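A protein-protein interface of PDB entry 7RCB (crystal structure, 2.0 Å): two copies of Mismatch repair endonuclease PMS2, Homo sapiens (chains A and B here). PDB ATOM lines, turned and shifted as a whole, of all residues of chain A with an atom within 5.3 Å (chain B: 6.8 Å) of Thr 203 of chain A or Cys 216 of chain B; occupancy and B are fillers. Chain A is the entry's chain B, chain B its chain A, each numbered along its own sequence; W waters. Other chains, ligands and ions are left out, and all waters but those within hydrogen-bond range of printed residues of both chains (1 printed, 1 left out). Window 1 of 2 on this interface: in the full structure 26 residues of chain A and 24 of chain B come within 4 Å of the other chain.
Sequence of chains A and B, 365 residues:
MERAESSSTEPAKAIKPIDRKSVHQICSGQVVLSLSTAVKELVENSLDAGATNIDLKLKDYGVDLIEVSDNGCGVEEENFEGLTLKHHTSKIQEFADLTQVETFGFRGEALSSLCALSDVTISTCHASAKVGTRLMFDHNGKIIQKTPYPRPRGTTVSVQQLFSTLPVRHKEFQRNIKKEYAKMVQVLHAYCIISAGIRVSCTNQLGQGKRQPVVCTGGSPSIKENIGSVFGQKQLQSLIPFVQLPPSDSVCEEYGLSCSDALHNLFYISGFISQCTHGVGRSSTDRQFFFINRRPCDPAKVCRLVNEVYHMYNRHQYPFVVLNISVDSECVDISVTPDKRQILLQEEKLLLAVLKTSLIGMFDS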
ATOM      1  N   LEU A  56      24.451   3.693   3.176  1.00  0.00           N
ATOM      2  CA  LEU A  56      25.192   3.760   1.927  1.00  0.00           C
ATOM      3  C   LEU A  56      24.199   4.091   0.824  1.00  0.00           C
ATOM      4  O   LEU A  56      23.288   3.306   0.550  1.00  0.00           O
ATOM      5  CB  LEU A  56      25.903   2.437   1.655  1.00  0.00           C
ATOM      6  CG  LEU A  56      26.521   2.262   0.272  1.00  0.00           C
ATOM      7  CD1 LEU A  56      27.591   3.309   0.023  1.00  0.00           C
ATOM      8  CD2 LEU A  56      27.089   0.865   0.132  1.00  0.00           C
ATOM      9  N   LYS A  57      24.378   5.244   0.191  1.00  0.00           N
ATOM     10  CA  LYS A  57      23.514   5.688  -0.893  1.00  0.00           C
ATOM     11  C   LYS A  57      24.298   5.645  -2.196  1.00  0.00           C
ATOM     12  O   LYS A  57      25.340   6.296  -2.323  1.00  0.00           O
ATOM     13  CB  LYS A  57      22.973   7.090  -0.621  1.00  0.00           C
ATOM     14  CG  LYS A  57      22.136   7.666  -1.749  1.00  0.00           C
ATOM     15  CD  LYS A  57      21.870   9.141  -1.523  1.00  0.00           C
ATOM     16  CE  LYS A  57      21.125   9.351  -0.221  1.00  0.00           C
ATOM     17  NZ  LYS A  57      20.606  10.736  -0.096  1.00  0.00           N
ATOM     18  N   LEU A  58      23.798   4.872  -3.153  1.00  0.00           N
ATOM     19  CA  LEU A  58      24.422   4.707  -4.455  1.00  0.00           C
ATOM     20  C   LEU A  58      23.544   5.287  -5.556  1.00  0.00           C
ATOM     21  O   LEU A  58      22.313   5.249  -5.480  1.00  0.00           O
ATOM     22  CB  LEU A  58      24.669   3.226  -4.749  1.00  0.00           C
ATOM     23  CG  LEU A  58      25.486   2.432  -3.734  1.00  0.00           C
ATOM     24  CD1 LEU A  58      25.464   0.967  -4.101  1.00  0.00           C
ATOM     25  CD2 LEU A  58      26.906   2.940  -3.707  1.00  0.00           C
ATOM     26  N   SER A 201      22.467   0.231   6.196  1.00  0.00           N
ATOM     27  CA  SER A 201      21.529   0.188   5.084  1.00  0.00           C
ATOM     28  C   SER A 201      22.225   0.606   3.803  1.00  0.00           C
ATOM     29  O   SER A 201      23.260   1.276   3.818  1.00  0.00           O
ATOM     30  CB  SER A 201      20.312   1.093   5.309  1.00  0.00           C
ATOM     31  OG  SER A 201      20.645   2.450   5.088  1.00  0.00           O
ATOM     32  N   CYS A 202      21.629   0.206   2.685  1.00  0.00           N
ATOM     33  CA  CYS A 202      22.114   0.572   1.367  1.00  0.00           C
ATOM     34  C   CYS A 202      20.924   0.765   0.443  1.00  0.00           C
ATOM     35  O   CYS A 202      19.974  -0.020   0.471  1.00  0.00           O
ATOM     36  CB  CYS A 202      23.050  -0.489   0.788  1.00  0.00           C
ATOM     37  SG  CYS A 202      23.634  -0.098  -0.873  1.00  0.00           S
ATOM     38  N   THR A 203      20.972   1.826  -0.355  1.00  0.00           N
ATOM     39  CA  THR A 203      19.977   2.076  -1.383  1.00  0.00           C
ATOM     40  C   THR A 203      20.699   2.356  -2.689  1.00  0.00           C
ATOM     41  O   THR A 203      21.874   2.735  -2.703  1.00  0.00           O
ATOM     42  CB  THR A 203      19.068   3.258  -1.033  1.00  0.00           C
ATOM     43  OG1 THR A 203      19.824   4.475  -1.096  1.00  0.00           O
ATOM     44  CG2 THR A 203      18.529   3.094   0.375  1.00  0.00           C
ATOM     45  N   ASN A 204      19.984   2.160  -3.789  1.00  0.00           N
ATOM     46  CA  ASN A 204      20.535   2.386  -5.115  1.00  0.00           C
ATOM     47  C   ASN A 204      19.477   3.038  -5.994  1.00  0.00           C
ATOM     48  O   ASN A 204      18.276   2.825  -5.805  1.00  0.00           O
ATOM     49  CB  ASN A 204      21.032   1.074  -5.730  1.00  0.00           C
ATOM     50  CG  ASN A 204      21.780   1.280  -7.025  1.00  0.00           C
ATOM     51  OD1 ASN A 204      22.371   2.333  -7.259  1.00  0.00           O
ATOM     52  ND2 ASN A 204      21.774   0.262  -7.873  1.00  0.00           N
ATOM     53  N   GLN A 205      19.932   3.882  -6.917  1.00  0.00           N
ATOM     54  CA  GLN A 205      19.045   4.577  -7.844  1.00  0.00           C
ATOM     55  C   GLN A 205      19.683   4.521  -9.227  1.00  0.00           C
ATOM     56  O   GLN A 205      20.838   4.919  -9.390  1.00  0.00           O
ATOM     57  CB  GLN A 205      18.804   6.018  -7.377  1.00  0.00           C
ATOM     58  CG  GLN A 205      17.849   6.842  -8.232  1.00  0.00           C
ATOM     59  CD  GLN A 205      17.592   8.220  -7.638  1.00  0.00           C
ATOM     60  OE1 GLN A 205      18.488   8.839  -7.066  1.00  0.00           O
ATOM     61  NE2 GLN A 205      16.353   8.695  -7.753  1.00  0.00           N
ATOM     62  N   LYS A 210      13.298   5.463  -9.696  1.00  0.00           N
ATOM     63  CA  LYS A 210      13.066   5.740  -8.289  1.00  0.00           C
ATOM     64  C   LYS A 210      14.146   5.093  -7.429  1.00  0.00           C
ATOM     65  O   LYS A 210      14.758   4.093  -7.812  1.00  0.00           O
ATOM     66  CB  LYS A 210      11.678   5.236  -7.888  1.00  0.00           C
ATOM     67  CG  LYS A 210      11.481   3.744  -8.087  1.00  0.00           C
ATOM     68  CD  LYS A 210      10.026   3.326  -7.859  1.00  0.00           C
ATOM     69  CE  LYS A 210       9.597   3.407  -6.396  1.00  0.00           C
ATOM     70  NZ  LYS A 210      10.337   2.429  -5.545  1.00  0.00           N
ATOM     71  N   ARG A 211      14.393   5.686  -6.263  1.00  0.00           N
ATOM     72  CA  ARG A 211      15.339   5.102  -5.321  1.00  0.00           C
ATOM     73  C   ARG A 211      14.785   3.801  -4.748  1.00  0.00           C
ATOM     74  O   ARG A 211      13.611   3.714  -4.378  1.00  0.00           O
ATOM     75  CB  ARG A 211      15.652   6.091  -4.198  1.00  0.00           C
ATOM     76  CG  ARG A 211      16.657   5.572  -3.185  1.00  0.00           C
ATOM     77  CD  ARG A 211      17.426   6.694  -2.504  1.00  0.00           C
ATOM     78  NE  ARG A 211      18.307   7.398  -3.430  1.00  0.00           N
ATOM     79  CZ  ARG A 211      19.474   6.936  -3.867  1.00  0.00           C
ATOM     80  NH1 ARG A 211      19.948   5.758  -3.483  1.00  0.00           N
ATOM     81  NH2 ARG A 211      20.189   7.681  -4.704  1.00  0.00           N
ATOM     82  N   GLN A 212      15.632   2.775  -4.692  1.00  0.00           N
ATOM     83  CA  GLN A 212      15.202   1.469  -4.234  1.00  0.00           C
ATOM     84  C   GLN A 212      16.053   0.976  -3.069  1.00  0.00           C
ATOM     85  O   GLN A 212      17.289   1.068  -3.123  1.00  0.00           O
ATOM     86  CB  GLN A 212      15.237   0.463  -5.392  1.00  0.00           C
ATOM     87  CG  GLN A 212      14.372   0.937  -6.554  1.00  0.00           C
ATOM     88  CD  GLN A 212      14.016  -0.154  -7.525  1.00  0.00           C
ATOM     89  OE1 GLN A 212      14.768  -1.105  -7.708  1.00  0.00           O
ATOM     90  NE2 GLN A 212      12.855  -0.025  -8.156  1.00  0.00           N
ATOM     91  N   PRO A 213      15.439   0.460  -2.006  1.00  0.00           N
ATOM     92  CA  PRO A 213      16.222  -0.125  -0.914  1.00  0.00           C
ATOM     93  C   PRO A 213      16.937  -1.385  -1.377  1.00  0.00           C
ATOM     94  O   PRO A 213      16.427  -2.149  -2.200  1.00  0.00           O
ATOM     95  CB  PRO A 213      15.176  -0.422   0.165  1.00  0.00           C
ATOM     96  CG  PRO A 213      13.870  -0.419  -0.537  1.00  0.00           C
ATOM     97  CD  PRO A 213      13.999   0.502  -1.705  1.00  0.00           C
ATOM     98  N   VAL A 214      18.148  -1.574  -0.865  1.00  0.00           N
ATOM     99  CA  VAL A 214      18.978  -2.727  -1.185  1.00  0.00           C
ATOM    100  C   VAL A 214      19.095  -3.672   0.005  1.00  0.00           C
ATOM    101  O   VAL A 214      18.869  -4.874  -0.125  1.00  0.00           O
ATOM    102  CB  VAL A 214      20.371  -2.285  -1.686  1.00  0.00           C
ATOM    103  CG1 VAL A 214      21.268  -3.496  -1.886  1.00  0.00           C
ATOM    104  CG2 VAL A 214      20.239  -1.499  -2.984  1.00  0.00           C
ATOM    105  N   CYS B 192       6.486  10.194   2.766  1.00  0.00           N
ATOM    106  CA  CYS B 192       7.787  10.235   2.105  1.00  0.00           C
ATOM    107  C   CYS B 192       8.038  11.595   1.475  1.00  0.00           C
ATOM    108  O   CYS B 192       9.131  12.160   1.601  1.00  0.00           O
ATOM    109  CB  CYS B 192       7.874   9.141   1.039  1.00  0.00           C
ATOM    110  SG  CYS B 192       8.170   7.484   1.675  1.00  0.00           S
ATOM    111  N   ARG B 199      15.073   9.734   6.151  1.00  0.00           N
ATOM    112  CA  ARG B 199      15.168   8.600   5.242  1.00  0.00           C
ATOM    113  C   ARG B 199      14.053   7.628   5.594  1.00  0.00           C
ATOM    114  O   ARG B 199      14.050   7.048   6.683  1.00  0.00           O
ATOM    115  CB  ARG B 199      16.532   7.925   5.348  1.00  0.00           C
ATOM    116  CG  ARG B 199      17.682   8.727   4.777  1.00  0.00           C
ATOM    117  CD  ARG B 199      19.021   8.079   5.112  1.00  0.00           C
ATOM    118  NE  ARG B 199      20.122   8.665   4.355  1.00  0.00           N
ATOM    119  CZ  ARG B 199      20.735   9.795   4.677  1.00  0.00           C
ATOM    120  NH1 ARG B 199      20.387  10.489   5.749  1.00  0.00           N
ATOM    121  NH2 ARG B 199      21.719  10.245   3.902  1.00  0.00           N
ATOM    122  N   VAL B 200      13.093   7.477   4.690  1.00  0.00           N
ATOM    123  CA  VAL B 200      12.001   6.525   4.850  1.00  0.00           C
ATOM    124  C   VAL B 200      12.185   5.445   3.800  1.00  0.00           C
ATOM    125  O   VAL B 200      12.397   5.752   2.624  1.00  0.00           O
ATOM    126  CB  VAL B 200      10.626   7.201   4.707  1.00  0.00           C
ATOM    127  CG1 VAL B 200       9.505   6.189   4.961  1.00  0.00           C
ATOM    128  CG2 VAL B 200      10.510   8.395   5.648  1.00  0.00           C
ATOM    129  N   SER B 201      12.127   4.187   4.222  1.00  0.00           N
ATOM    130  CA  SER B 201      12.261   3.075   3.294  1.00  0.00           C
ATOM    131  C   SER B 201      11.198   2.035   3.609  1.00  0.00           C
ATOM    132  O   SER B 201      10.741   1.910   4.748  1.00  0.00           O
ATOM    133  CB  SER B 201      13.661   2.447   3.356  1.00  0.00           C
ATOM    134  OG  SER B 201      13.823   1.655   4.520  1.00  0.00           O
ATOM    135  N   CYS B 202      10.815   1.279   2.585  1.00  0.00           N
ATOM    136  CA  CYS B 202       9.809   0.246   2.755  1.00  0.00           C
ATOM    137  C   CYS B 202      10.082  -0.895   1.792  1.00  0.00           C
ATOM    138  O   CYS B 202      10.406  -0.669   0.625  1.00  0.00           O
ATOM    139  CB  CYS B 202       8.400   0.800   2.530  1.00  0.00           C
ATOM    140  SG  CYS B 202       7.099  -0.432   2.707  1.00  0.00           S
ATOM    141  N   PRO B 213      11.474  -3.844  -3.297  1.00  0.00           N
ATOM    142  CA  PRO B 213      11.433  -2.422  -2.945  1.00  0.00           C
ATOM    143  C   PRO B 213      10.049  -1.843  -3.168  1.00  0.00           C
ATOM    144  O   PRO B 213       9.379  -2.142  -4.157  1.00  0.00           O
ATOM    145  CB  PRO B 213      12.455  -1.785  -3.896  1.00  0.00           C
ATOM    146  CG  PRO B 213      12.610  -2.749  -5.006  1.00  0.00           C
ATOM    147  CD  PRO B 213      12.347  -4.113  -4.450  1.00  0.00           C
ATOM    148  N   VAL B 214       9.620  -1.006  -2.237  1.00  0.00           N
ATOM    149  CA  VAL B 214       8.346  -0.314  -2.336  1.00  0.00           C
ATOM    150  C   VAL B 214       8.550   1.185  -2.518  1.00  0.00           C
ATOM    151  O   VAL B 214       8.058   1.774  -3.480  1.00  0.00           O
ATOM    152  CB  VAL B 214       7.456  -0.610  -1.108  1.00  0.00           C
ATOM    153  CG1 VAL B 214       6.175   0.217  -1.162  1.00  0.00           C
ATOM    154  CG2 VAL B 214       7.133  -2.095  -1.029  1.00  0.00           C
ATOM    155  N   VAL B 215       9.299   1.813  -1.610  1.00  0.00           N
ATOM    156  CA  VAL B 215       9.605   3.238  -1.697  1.00  0.00           C
ATOM    157  C   VAL B 215      10.836   3.497  -0.842  1.00  0.00           C
ATOM    158  O   VAL B 215      11.148   2.737   0.075  1.00  0.00           O
ATOM    159  CB  VAL B 215       8.401   4.108  -1.247  1.00  0.00           C
ATOM    160  CG1 VAL B 215       8.230   4.056   0.261  1.00  0.00           C
ATOM    161  CG2 VAL B 215       8.567   5.548  -1.720  1.00  0.00           C
ATOM    162  N   CYS B 216      11.548   4.577  -1.147  1.00  0.00           N
ATOM    163  CA  CYS B 216      12.772   4.891  -0.421  1.00  0.00           C
ATOM    164  C   CYS B 216      13.148   6.342  -0.670  1.00  0.00           C
ATOM    165  O   CYS B 216      13.305   6.744  -1.828  1.00  0.00           O
ATOM    166  CB  CYS B 216      13.888   3.962  -0.863  1.00  0.00           C
ATOM    167  SG  CYS B 216      15.365   4.162   0.076  1.00  0.00           S
ATOM    168  N   THR B 217      13.267   7.131   0.394  1.00  0.00           N
ATOM    169  CA  THR B 217      13.810   8.478   0.302  1.00  0.00           C
ATOM    170  C   THR B 217      15.262   8.507   0.775  1.00  0.00           C
ATOM    171  O   THR B 217      15.722   7.632   1.510  1.00  0.00           O
ATOM    172  CB  THR B 217      12.962   9.473   1.098  1.00  0.00           C
ATOM    173  OG1 THR B 217      12.902   9.077   2.474  1.00  0.00           O
ATOM    174  CG2 THR B 217      11.560   9.526   0.526  1.00  0.00           C
ATOM    175  N   GLY B 218      15.979   9.539   0.342  1.00  0.00           N
ATOM    176  CA  GLY B 218      17.402   9.662   0.578  1.00  0.00           C
ATOM    177  C   GLY B 218      17.826  10.620   1.668  1.00  0.00           C
ATOM    178  O   GLY B 218      19.020  10.930   1.762  1.00  0.00           O
ATOM    179  N   ASN B 226      12.607  14.617  -2.638  1.00  0.00           N
ATOM    180  CA  ASN B 226      11.830  13.469  -2.183  1.00  0.00           C
ATOM    181  C   ASN B 226      10.916  12.954  -3.285  1.00  0.00           C
ATOM    182  O   ASN B 226      10.737  11.741  -3.435  1.00  0.00           O
ATOM    183  CB  ASN B 226      11.011  13.833  -0.945  1.00  0.00           C
ATOM    184  CG  ASN B 226      11.839  13.846   0.325  1.00  0.00           C
ATOM    185  OD1 ASN B 226      12.932  13.277   0.378  1.00  0.00           O
ATOM    186  ND2 ASN B 226      11.315  14.486   1.359  1.00  0.00           N
ATOM    187  N   GLY B 228      11.545  13.084  -6.482  1.00  0.00           N
ATOM    188  CA  GLY B 228      12.414  12.314  -7.356  1.00  0.00           C
ATOM    189  C   GLY B 228      12.744  10.944  -6.796  1.00  0.00           C
ATOM    190  O   GLY B 228      12.766   9.956  -7.528  1.00  0.00           O
ATOM    191  N   SER B 229      12.997  10.863  -5.488  1.00  0.00           N
ATOM    192  CA  SER B 229      13.266   9.565  -4.872  1.00  0.00           C
ATOM    193  C   SER B 229      12.056   8.639  -4.961  1.00  0.00           C
ATOM    194  O   SER B 229      12.198   7.445  -5.254  1.00  0.00           O
ATOM    195  CB  SER B 229      13.686   9.750  -3.416  1.00  0.00           C
ATOM    196  OG  SER B 229      14.926  10.426  -3.320  1.00  0.00           O
ATOM    197  N   VAL B 230      10.857   9.176  -4.730  1.00  0.00           N
ATOM    198  CA  VAL B 230       9.665   8.338  -4.650  1.00  0.00           C
ATOM    199  C   VAL B 230       9.241   7.867  -6.036  1.00  0.00           C
ATOM    200  O   VAL B 230       8.913   6.692  -6.230  1.00  0.00           O
ATOM    201  CB  VAL B 230       8.532   9.096  -3.927  1.00  0.00           C
ATOM    202  CG1 VAL B 230       7.227   8.321  -4.008  1.00  0.00           C
ATOM    203  CG2 VAL B 230       8.896   9.339  -2.473  1.00  0.00           C
HETATM  204  O   HOH W   1      11.368   4.954  -4.274  1.00  0.00           O
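N of Cys 202 of chain B sits at hydrogen-bond distance from O of Val 215 of chain B (2.9 Å).
N of Leu 58 of chain A sits at hydrogen-bond distance from O of Thr 203 of chain A.
The backbone carbonyl oxygen of Cys 202 of chain B is in hydrogen-bond range of the backbone NH of Val 214 of chain B (3.0 Å).
O of Leu 58 of chain A sits at hydrogen-bond distance from N of Gln 205 of chain A (3.1 Å).
The backbone NH (N) of Thr 203 of chain A is in hydrogen-bond range of the backbone carbonyl oxygen (O) of Leu 56 of chain A (2.9 Å).
O of Leu 58 of chain A lies within hydrogen-bond range of NH1 of Arg 211 of chain A (3.1 Å).
The backbone carbonyl oxygen (O) of Ser 229 of chain B is in hydrogen-bond range of the backbone NH (N) of Arg 211 of chain A (3.0 Å).
The side-chain amino group of Lys 210 of chain A sits at hydrogen-bond distance from the backbone carbonyl oxygen of Val 214 of chain B.
O of Gly 218 of chain B is in hydrogen-bond range of NZ of Lys 57 of chain A.
Cys 216 of chain B touches Thr 203 of chain A.
Gln 205 of chain A touches Gly 228 of chain B.
Val 215 of chain B touches Lys 210 of chain A (CA to NZ, 3.9997 Å).
CB of Lys 210 of chain A touches O of Ser 229 of chain B (3.5 Å).
O of Val 230 of chain B touches CE of Lys 210 of chain A, at 3.4 Å.
CB of Arg 211 of chain A touches O of Cys 216 of chain B, 3.4 Å away.
CG of Pro 213 of chain B touches OE1 of Gln 212 of chain A, at 3.8 Å.
Pro 213 of chain A touches Cys 202 of chain B.
CB of Pro 213 of chain B touches CD of Pro 213 of chain A (3.5 Å).
CB of Cys 216 of chain B touches CD of Pro 213 of chain A, at 3.6 Å.
Pro 213 of chain A touches Cys 202 of chain B, but with the chains exchanged Cys 202 of chain A does not touch Pro 213 of chain B (8.9 Å).
Pro 213 of chain A touches its own counterpart, Pro 213 of chain B.
4 positions are printed for both chains.
Thr 203 of chain A touches just one residue of chain B: Cys 216.
Of chain A, only Thr 203 (3.4 Å), Arg 211 (3.4 Å) and Pro 213 (3.6 Å) come within 4 Å of Cys 216 of chain B.
Printed residues of chain A within 4 Å of Val 214 of chain B: Lys 210.
Of the printed residues of chain B, Arg 211 of chain A touches Cys 216 (3.4 Å) and Ser 229 (3.0 Å).
Printed residues of chain A within 4 Å of Gly 218 of chain B: Lys 57.
The nearest residue of chain B that does not touch Thr 203 of chain A is Thr 217 of chain B (5.5 Å).
Of the 13 printed residues of chain A, 7 touch a printed residue of chain B.
Hydrophobic or aromatic side chains of chain A within 4 Å of the printed part of chain B: Pro 213.
Of the 15 printed residues of chain B, 9 touch a printed residue of chain A.
Hydrophobic or aromatic side chains of chain B within 4 Å of the printed part of chain A: Pro 213.
Among the printed residues, 13 pairs touch across the chains.
Water W1 lies within hydrogen-bond range of the backbone carbonyl oxygen (O) of Arg 211 of chain A, the backbone carbonyl oxygen (O) of Ser 229 of chain B, the side-chain amino group (NZ) of Lys 210 of chain A and the backbone NH (N) of Cys 216 of chain B.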
